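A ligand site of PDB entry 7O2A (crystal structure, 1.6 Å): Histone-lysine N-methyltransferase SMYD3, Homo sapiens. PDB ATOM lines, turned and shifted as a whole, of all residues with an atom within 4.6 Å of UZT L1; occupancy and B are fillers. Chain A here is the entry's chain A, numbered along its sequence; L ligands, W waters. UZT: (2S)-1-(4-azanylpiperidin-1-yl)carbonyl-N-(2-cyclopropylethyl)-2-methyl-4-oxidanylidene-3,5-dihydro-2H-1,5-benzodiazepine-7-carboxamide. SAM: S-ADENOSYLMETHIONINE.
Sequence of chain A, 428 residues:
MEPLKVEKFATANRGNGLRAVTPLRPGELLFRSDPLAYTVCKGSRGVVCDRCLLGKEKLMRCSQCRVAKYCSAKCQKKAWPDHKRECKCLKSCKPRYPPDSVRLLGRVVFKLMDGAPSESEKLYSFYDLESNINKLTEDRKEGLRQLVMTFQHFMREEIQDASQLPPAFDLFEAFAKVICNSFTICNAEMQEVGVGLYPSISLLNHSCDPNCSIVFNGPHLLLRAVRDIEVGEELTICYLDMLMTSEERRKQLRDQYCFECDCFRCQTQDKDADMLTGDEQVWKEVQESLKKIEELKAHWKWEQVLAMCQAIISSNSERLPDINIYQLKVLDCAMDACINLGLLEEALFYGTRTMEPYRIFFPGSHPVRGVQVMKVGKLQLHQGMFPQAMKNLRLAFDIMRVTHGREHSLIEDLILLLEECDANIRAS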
ATOM      1  N   CYS A 180      23.087  -9.984 -19.394  1.00  0.00           N
ATOM      2  CA  CYS A 180      24.476  -9.925 -19.016  1.00  0.00           C
ATOM      3  C   CYS A 180      25.205  -8.664 -19.502  1.00  0.00           C
ATOM      4  O   CYS A 180      26.411  -8.583 -19.300  1.00  0.00           O
ATOM      5  CB  CYS A 180      25.216 -11.166 -19.418  1.00  0.00           C
ATOM      6  SG  CYS A 180      25.294 -11.408 -21.221  1.00  0.00           S
ATOM      7  N   ASN A 181      24.486  -7.719 -20.114  1.00  0.00           N
ATOM      8  CA  ASN A 181      25.078  -6.434 -20.518  1.00  0.00           C
ATOM      9  C   ASN A 181      24.356  -5.192 -20.012  1.00  0.00           C
ATOM     10  O   ASN A 181      24.750  -4.100 -20.340  1.00  0.00           O
ATOM     11  CB  ASN A 181      25.138  -6.364 -22.018  1.00  0.00           C
ATOM     12  CG  ASN A 181      26.058  -7.374 -22.615  1.00  0.00           C
ATOM     13  OD1 ASN A 181      27.241  -7.186 -22.597  1.00  0.00           O
ATOM     14  ND2 ASN A 181      25.526  -8.474 -23.112  1.00  0.00           N
ATOM     15  N   SER A 182      23.322  -5.306 -19.206  1.00  0.00           N
ATOM     16  CA  SER A 182      22.686  -4.097 -18.656  1.00  0.00           C
ATOM     17  C   SER A 182      23.557  -3.398 -17.644  1.00  0.00           C
ATOM     18  O   SER A 182      24.048  -4.061 -16.768  1.00  0.00           O
ATOM     19  CB  SER A 182      21.434  -4.475 -17.875  1.00  0.00           C
ATOM     20  OG  SER A 182      20.470  -4.841 -18.777  1.00  0.00           O
ATOM     21  N   PHE A 183      23.595  -2.077 -17.714  1.00  0.00           N
ATOM     22  CA  PHE A 183      24.250  -1.265 -16.717  1.00  0.00           C
ATOM     23  C   PHE A 183      23.215  -0.667 -15.777  1.00  0.00           C
ATOM     24  O   PHE A 183      22.237  -0.102 -16.180  1.00  0.00           O
ATOM     25  CB  PHE A 183      25.112  -0.171 -17.367  1.00  0.00           C
ATOM     26  CG  PHE A 183      26.350  -0.673 -18.026  1.00  0.00           C
ATOM     27  CD1 PHE A 183      27.558  -0.620 -17.373  1.00  0.00           C
ATOM     28  CD2 PHE A 183      26.305  -1.244 -19.262  1.00  0.00           C
ATOM     29  CE1 PHE A 183      28.706  -1.070 -17.985  1.00  0.00           C
ATOM     30  CE2 PHE A 183      27.493  -1.682 -19.870  1.00  0.00           C
ATOM     31  CZ  PHE A 183      28.670  -1.635 -19.199  1.00  0.00           C
ATOM     32  N   THR A 184      23.540  -0.743 -14.479  1.00  0.00           N
ATOM     33  CA  THR A 184      22.729  -0.070 -13.464  1.00  0.00           C
ATOM     34  C   THR A 184      23.175   1.398 -13.285  1.00  0.00           C
ATOM     35  O   THR A 184      24.304   1.659 -12.890  1.00  0.00           O
ATOM     36  CB  THR A 184      22.895  -0.794 -12.099  1.00  0.00           C
ATOM     37  OG1 THR A 184      22.487  -2.181 -12.227  1.00  0.00           O
ATOM     38  CG2 THR A 184      22.044  -0.147 -11.071  1.00  0.00           C
ATOM     39  N   ILE A 185      22.279   2.352 -13.609  1.00  0.00           N
ATOM     40  CA  ILE A 185      22.596   3.786 -13.571  1.00  0.00           C
ATOM     41  C   ILE A 185      22.272   4.288 -12.160  1.00  0.00           C
ATOM     42  O   ILE A 185      21.089   4.200 -11.736  1.00  0.00           O
ATOM     43  CB  ILE A 185      21.758   4.574 -14.627  1.00  0.00           C
ATOM     44  CG1 ILE A 185      21.996   3.993 -15.993  1.00  0.00           C
ATOM     45  CG2 ILE A 185      22.135   6.050 -14.564  1.00  0.00           C
ATOM     46  CD1 ILE A 185      21.017   4.405 -17.060  1.00  0.00           C
ATOM     47  N   CYS A 186      23.267   4.805 -11.435  1.00  0.00           N
ATOM     48  CA  CYS A 186      23.000   5.480 -10.171  1.00  0.00           C
ATOM     49  C   CYS A 186      23.171   6.965 -10.307  1.00  0.00           C
ATOM     50  O   CYS A 186      23.936   7.481 -11.156  1.00  0.00           O
ATOM     51  CB  CYS A 186      23.919   4.952  -9.056  1.00  0.00           C
ATOM     52  SG  CYS A 186      23.742   3.191  -8.730  1.00  0.00           S
ATOM     53  N   MET A 190      24.569   8.029  -5.534  1.00  0.00           N
ATOM     54  CA  MET A 190      24.687   6.565  -5.665  1.00  0.00           C
ATOM     55  C   MET A 190      23.393   5.797  -5.409  1.00  0.00           C
ATOM     56  O   MET A 190      23.431   4.624  -5.128  1.00  0.00           O
ATOM     57  CB  MET A 190      25.862   6.007  -4.872  1.00  0.00           C
ATOM     58  CG  MET A 190      27.228   6.410  -5.434  1.00  0.00           C
ATOM     59  SD  MET A 190      27.457   5.648  -7.060  1.00  0.00           S
ATOM     60  CE  MET A 190      29.052   6.383  -7.425  1.00  0.00           C
ATOM     61  N   GLU A 192      20.299   4.033  -6.986  1.00  0.00           N
ATOM     62  CA  GLU A 192      19.840   3.458  -8.271  1.00  0.00           C
ATOM     63  C   GLU A 192      18.682   4.228  -8.861  1.00  0.00           C
ATOM     64  O   GLU A 192      17.646   4.422  -8.202  1.00  0.00           O
ATOM     65  CB  GLU A 192      19.374   2.023  -8.145  1.00  0.00           C
ATOM     66  CG  GLU A 192      20.423   1.032  -7.861  1.00  0.00           C
ATOM     67  CD  GLU A 192      19.892  -0.418  -7.904  1.00  0.00           C
ATOM     68  OE1 GLU A 192      18.898  -0.655  -8.631  1.00  0.00           O
ATOM     69  OE2 GLU A 192      20.502  -1.247  -7.187  1.00  0.00           O
ATOM     70  N   ILE A 214      33.547   2.710 -13.464  1.00  0.00           N
ATOM     71  CA  ILE A 214      32.543   3.511 -14.142  1.00  0.00           C
ATOM     72  C   ILE A 214      31.754   4.403 -13.142  1.00  0.00           C
ATOM     73  O   ILE A 214      31.470   4.001 -11.983  1.00  0.00           O
ATOM     74  CB  ILE A 214      31.568   2.694 -14.945  1.00  0.00           C
ATOM     75  CG1 ILE A 214      30.771   1.694 -14.062  1.00  0.00           C
ATOM     76  CG2 ILE A 214      32.268   2.003 -16.094  1.00  0.00           C
ATOM     77  CD1 ILE A 214      29.674   0.973 -14.875  1.00  0.00           C
ATOM     78  N   PHE A 216      28.332   7.449 -13.348  1.00  0.00           N
ATOM     79  CA  PHE A 216      27.275   8.043 -14.127  1.00  0.00           C
ATOM     80  C   PHE A 216      27.045   9.467 -13.701  1.00  0.00           C
ATOM     81  O   PHE A 216      27.038   9.772 -12.511  1.00  0.00           O
ATOM     82  CB  PHE A 216      25.995   7.239 -13.993  1.00  0.00           C
ATOM     83  CG  PHE A 216      26.101   5.849 -14.579  1.00  0.00           C
ATOM     84  CD1 PHE A 216      25.748   5.566 -15.930  1.00  0.00           C
ATOM     85  CD2 PHE A 216      26.507   4.776 -13.771  1.00  0.00           C
ATOM     86  CE1 PHE A 216      25.892   4.277 -16.427  1.00  0.00           C
ATOM     87  CE2 PHE A 216      26.658   3.528 -14.303  1.00  0.00           C
ATOM     88  CZ  PHE A 216      26.346   3.288 -15.641  1.00  0.00           C
ATOM     89  N   ILE A 237      36.351  -3.850 -14.852  1.00  0.00           N
ATOM     90  CA  ILE A 237      35.599  -3.206 -13.806  1.00  0.00           C
ATOM     91  C   ILE A 237      35.012  -4.295 -12.934  1.00  0.00           C
ATOM     92  O   ILE A 237      34.930  -5.441 -13.351  1.00  0.00           O
ATOM     93  CB  ILE A 237      34.417  -2.318 -14.386  1.00  0.00           C
ATOM     94  CG1 ILE A 237      33.418  -3.158 -15.232  1.00  0.00           C
ATOM     95  CG2 ILE A 237      35.070  -1.129 -15.111  1.00  0.00           C
ATOM     96  CD1 ILE A 237      32.231  -2.336 -15.618  1.00  0.00           C
ATOM     97  N   CYS A 238      34.584  -3.975 -11.733  1.00  0.00           N
ATOM     98  CA  CYS A 238      33.855  -4.913 -10.900  1.00  0.00           C
ATOM     99  C   CYS A 238      32.372  -4.760 -11.261  1.00  0.00           C
ATOM    100  O   CYS A 238      31.786  -3.674 -11.124  1.00  0.00           O
ATOM    101  CB  CYS A 238      34.127  -4.621  -9.404  1.00  0.00           C
ATOM    102  SG  CYS A 238      33.344  -5.914  -8.396  1.00  0.00           S
ATOM    103  N   TYR A 239      31.765  -5.844 -11.752  1.00  0.00           N
ATOM    104  CA  TYR A 239      30.354  -5.815 -12.099  1.00  0.00           C
ATOM    105  C   TYR A 239      29.428  -5.671 -10.871  1.00  0.00           C
ATOM    106  O   TYR A 239      28.208  -5.364 -11.025  1.00  0.00           O
ATOM    107  CB  TYR A 239      29.910  -7.074 -12.835  1.00  0.00           C
ATOM    108  CG  TYR A 239      30.492  -7.300 -14.217  1.00  0.00           C
ATOM    109  CD1 TYR A 239      31.323  -6.411 -14.832  1.00  0.00           C
ATOM    110  CD2 TYR A 239      30.148  -8.456 -14.918  1.00  0.00           C
ATOM    111  CE1 TYR A 239      31.809  -6.642 -16.128  1.00  0.00           C
ATOM    112  CE2 TYR A 239      30.634  -8.716 -16.179  1.00  0.00           C
ATOM    113  CZ  TYR A 239      31.473  -7.810 -16.753  1.00  0.00           C
ATOM    114  OH  TYR A 239      31.894  -8.094 -18.027  1.00  0.00           O
ATOM    115  N   ASP A 241      28.370  -5.051  -6.565  1.00  0.00           N
ATOM    116  CA  ASP A 241      28.513  -4.520  -5.217  1.00  0.00           C
ATOM    117  C   ASP A 241      29.720  -5.079  -4.499  1.00  0.00           C
ATOM    118  O   ASP A 241      29.919  -6.234  -4.485  1.00  0.00           O
ATOM    119  CB  ASP A 241      27.228  -4.911  -4.505  1.00  0.00           C
ATOM    120  CG  ASP A 241      27.133  -4.556  -3.027  1.00  0.00           C
ATOM    121  OD1 ASP A 241      27.888  -3.681  -2.492  1.00  0.00           O
ATOM    122  OD2 ASP A 241      26.254  -5.296  -2.382  1.00  0.00           O
ATOM    123  N   TYR A 257      25.833 -13.931 -15.242  1.00  0.00           N
ATOM    124  CA  TYR A 257      26.930 -13.744 -16.189  1.00  0.00           C
ATOM    125  C   TYR A 257      27.504 -15.013 -16.790  1.00  0.00           C
ATOM    126  O   TYR A 257      28.389 -14.951 -17.611  1.00  0.00           O
ATOM    127  CB  TYR A 257      28.024 -12.827 -15.596  1.00  0.00           C
ATOM    128  CG  TYR A 257      27.499 -11.426 -15.268  1.00  0.00           C
ATOM    129  CD1 TYR A 257      27.306 -10.477 -16.285  1.00  0.00           C
ATOM    130  CD2 TYR A 257      27.196 -11.058 -13.974  1.00  0.00           C
ATOM    131  CE1 TYR A 257      26.801  -9.278 -16.025  1.00  0.00           C
ATOM    132  CE2 TYR A 257      26.708  -9.795 -13.700  1.00  0.00           C
ATOM    133  CZ  TYR A 257      26.528  -8.918 -14.731  1.00  0.00           C
ATOM    134  OH  TYR A 257      25.985  -7.615 -14.519  1.00  0.00           O
ATOM    135  N   HIS A 366      37.654   4.064  -5.315  1.00  0.00           N
ATOM    136  CA  HIS A 366      36.383   3.506  -5.738  1.00  0.00           C
ATOM    137  C   HIS A 366      35.343   4.627  -5.556  1.00  0.00           C
ATOM    138  O   HIS A 366      35.264   5.260  -4.514  1.00  0.00           O
ATOM    139  CB  HIS A 366      35.990   2.303  -4.810  1.00  0.00           C
ATOM    140  CG  HIS A 366      34.821   1.515  -5.310  1.00  0.00           C
ATOM    141  ND1 HIS A 366      33.567   2.059  -5.450  1.00  0.00           N
ATOM    142  CD2 HIS A 366      34.725   0.248  -5.816  1.00  0.00           C
ATOM    143  CE1 HIS A 366      32.719   1.134  -5.860  1.00  0.00           C
ATOM    144  NE2 HIS A 366      33.401   0.038  -6.160  1.00  0.00           N
ATOM    145  N   PRO A 367      34.472   4.851  -6.561  1.00  0.00           N
ATOM    146  CA  PRO A 367      33.509   5.962  -6.473  1.00  0.00           C
ATOM    147  C   PRO A 367      32.551   5.940  -5.307  1.00  0.00           C
ATOM    148  O   PRO A 367      32.138   6.994  -4.805  1.00  0.00           O
ATOM    149  CB  PRO A 367      32.810   5.925  -7.829  1.00  0.00           C
ATOM    150  CG  PRO A 367      32.962   4.492  -8.282  1.00  0.00           C
ATOM    151  CD  PRO A 367      34.322   4.084  -7.814  1.00  0.00           C
ATOM    152  N   VAL A 368      32.142   4.738  -4.872  1.00  0.00           N
ATOM    153  CA  VAL A 368      31.180   4.612  -3.803  1.00  0.00           C
ATOM    154  C   VAL A 368      31.792   5.132  -2.503  1.00  0.00           C
ATOM    155  O   VAL A 368      31.111   5.781  -1.759  1.00  0.00           O
ATOM    156  CB  VAL A 368      30.680   3.160  -3.709  1.00  0.00           C
ATOM    157  CG1 VAL A 368      29.987   2.862  -2.378  1.00  0.00           C
ATOM    158  CG2 VAL A 368      29.788   2.896  -4.902  1.00  0.00           C
HETATM  159  C4  UZT L   1      28.166  -4.064 -15.662  1.00  0.00           C
HETATM  160  C5  UZT L   1      27.213  -4.470 -14.546  1.00  0.00           C
HETATM  161  C7  UZT L   1      26.888  -2.377 -13.292  1.00  0.00           C
HETATM  162  C10 UZT L   1      27.767  -2.064 -10.935  1.00  0.00           C
HETATM  163  C13 UZT L   1      26.860   0.612 -10.959  1.00  0.00           C
HETATM  164  C17 UZT L   1      28.498   2.796 -10.074  1.00  0.00           C
HETATM  165  C20 UZT L   1      29.966   1.545  -8.543  1.00  0.00           C
HETATM  166  C21 UZT L   1      27.269   0.325  -7.511  1.00  0.00           C
HETATM  167  C24 UZT L   1      25.543  -1.206  -8.433  1.00  0.00           C
HETATM  168  C26 UZT L   1      23.718  -1.383  -6.563  1.00  0.00           C
HETATM  169  C28 UZT L   1      26.102  -1.195  -6.052  1.00  0.00           C
HETATM  170  C1  UZT L   1      28.774  -4.804 -18.051  1.00  0.00           C
HETATM  171  C2  UZT L   1      28.019  -6.012 -17.413  1.00  0.00           C
HETATM  172  C3  UZT L   1      27.672  -4.581 -17.052  1.00  0.00           C
HETATM  173  N6  UZT L   1      27.321  -3.635 -13.313  1.00  0.00           N
HETATM  174  O8  UZT L   1      26.265  -1.901 -14.236  1.00  0.00           O
HETATM  175  C9  UZT L   1      27.126  -1.549 -12.079  1.00  0.00           C
HETATM  176  C14 UZT L   1      26.692  -0.228 -12.070  1.00  0.00           C
HETATM  177  C11 UZT L   1      27.947  -1.199  -9.826  1.00  0.00           C
HETATM  178  C12 UZT L   1      27.418   0.156  -9.826  1.00  0.00           C
HETATM  179  N15 UZT L   1      26.370   1.861 -11.005  1.00  0.00           N
HETATM  180  C16 UZT L   1      27.061   2.929 -10.555  1.00  0.00           C
HETATM  181  O30 UZT L   1      26.501   4.014 -10.603  1.00  0.00           O
HETATM  182  C18 UZT L   1      28.581   2.004  -8.697  1.00  0.00           C
HETATM  183  N19 UZT L   1      27.654   0.835  -8.672  1.00  0.00           N
HETATM  184  O22 UZT L   1      27.681   0.793  -6.418  1.00  0.00           O
HETATM  185  N23 UZT L   1      26.291  -0.590  -7.376  1.00  0.00           N
HETATM  186  C25 UZT L   1      24.172  -0.700  -7.958  1.00  0.00           C
HETATM  187  N29 UZT L   1      22.559  -0.693  -5.933  1.00  0.00           N
HETATM  188  C27 UZT L   1      24.749  -1.291  -5.481  1.00  0.00           C
HETATM  189  N   SAM L   2      33.449 -10.889 -22.760  1.00  0.00           N
HETATM  190  CA  SAM L   2      32.298 -10.111 -23.233  1.00  0.00           C
HETATM  191  C   SAM L   2      32.107 -10.198 -24.732  1.00  0.00           C
HETATM  192  O   SAM L   2      32.764 -11.040 -25.363  1.00  0.00           O
HETATM  193  OXT SAM L   2      31.238  -9.467 -25.227  1.00  0.00           O
HETATM  194  CB  SAM L   2      32.382  -8.670 -22.740  1.00  0.00           C
HETATM  195  CG  SAM L   2      31.808  -8.477 -21.322  1.00  0.00           C
HETATM  196  SD  SAM L   2      30.100  -8.753 -21.136  1.00  0.00           S
HETATM  197  CE  SAM L   2      29.475  -7.384 -20.366  1.00  0.00           C
HETATM  198  C5' SAM L   2      29.858  -9.982 -19.922  1.00  0.00           C
HETATM  199  C4' SAM L   2      30.302 -11.394 -20.225  1.00  0.00           C
HETATM  200  O4' SAM L   2      31.711 -11.457 -20.399  1.00  0.00           O
HETATM  201  C3' SAM L   2      30.036 -12.428 -19.111  1.00  0.00           C
HETATM  202  O3' SAM L   2      28.649 -12.808 -19.069  1.00  0.00           O
HETATM  203  C2' SAM L   2      30.957 -13.545 -19.483  1.00  0.00           C
HETATM  204  O2' SAM L   2      30.566 -14.211 -20.680  1.00  0.00           O
HETATM  205  C1' SAM L   2      32.194 -12.682 -19.818  1.00  0.00           C
HETATM  206  N9  SAM L   2      33.027 -12.331 -18.630  1.00  0.00           N
HETATM  207  C8  SAM L   2      33.155 -11.121 -18.049  1.00  0.00           C
HETATM  208  N7  SAM L   2      34.085 -11.142 -17.101  1.00  0.00           N
HETATM  209  C5  SAM L   2      34.639 -12.367 -17.122  1.00  0.00           C
HETATM  210  C6  SAM L   2      35.637 -13.045 -16.366  1.00  0.00           C
HETATM  211  N6  SAM L   2      36.332 -12.427 -15.406  1.00  0.00           N
HETATM  212  N1  SAM L   2      35.849 -14.322 -16.626  1.00  0.00           N
HETATM  213  C2  SAM L   2      35.211 -14.986 -17.583  1.00  0.00           C
HETATM  214  N3  SAM L   2      34.256 -14.452 -18.340  1.00  0.00           N
HETATM  215  C4  SAM L   2      33.953 -13.171 -18.119  1.00  0.00           C
HETATM  216  O   HOH W   1      28.001   6.389 -10.640  1.00  0.00           O
HETATM  217  O   HOH W   2      24.074   2.193  -5.502  1.00  0.00           O
HETATM  218  O   HOH W   3      23.777  -3.350 -10.012  1.00  0.00           O
HETATM  219  O   HOH W   4      26.373   2.009  -4.175  1.00  0.00           O
HETATM  220  O   HOH W   5      29.784  -0.934  -5.182  1.00  0.00           O
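A ring nitrogen (ND1) of His 366 lies within hydrogen-bond range of the backbone NH (N) of Val 368 (3.1 Å). ND2 of Asn 181 lies within hydrogen-bond range of SG of Cys 180, at 3.5 Å.
Cys 180 touches UZT L1. Ser 182 touches UZT L1 (O to C3, 3.7 Å). Phe 183 touches UZT L1 (CA to O8, 3.3 Å). O of Ile 214 touches C17 of UZT L1 (3.7 Å). CD2 of Phe 216 touches O30 of UZT L1, 3.3 Å away. OH of Tyr 257 touches C5 of UZT L1, at 3.4 Å. CE1 of His 366 touches C20 of UZT L1, 3.9 Å away. Val 368 touches UZT L1 (CG2 to O22, 3.3 Å). Hydrophobic or aromatic side chains that line UZT L1: Phe 183, Phe 216, Tyr 239, Tyr 257, His 366 and Val 368. Of the 19 residues printed, 12 come within 4 Å of UZT L1.
OE2 of Glu 192 is in salt-bridge range of N29 of UZT L1. N of Thr 184 is in hydrogen-bond range of O8 of UZT L1, at 3.0 Å. The backbone carbonyl oxygen (O) of Thr 184 is in hydrogen-bond range of a nitrogen (N15) of UZT L1, at 2.8 Å. O of Tyr 239 sits at hydrogen-bond distance from N6 of UZT L1 (3.0 Å). The backbone NH of Cys 186 lies close to an oxygen (O30) of UZT L1 (3.4 Å). The side-chain sulfur (SG) of Cys 186 sits close to an oxygen (O30) of UZT L1, at 3.4 Å. The backbone carbonyl oxygen of Tyr 257 lies within hydrogen-bond range of an oxygen (O3') of SAM L2 (2.6 Å).
Water W1 lies within hydrogen-bond range of an oxygen (O30) of UZT L1 (2.8 Å), the backbone NH (N) of Phe 216 (2.9 Å) and the side-chain sulfur (SD) of Met 190 (3.7 Å). Water W2 lies within hydrogen-bond range of O of Met 190 (2.5 Å), N29 of UZT L1 (3.3 Å) and SG of Cys 186 (3.4 Å).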
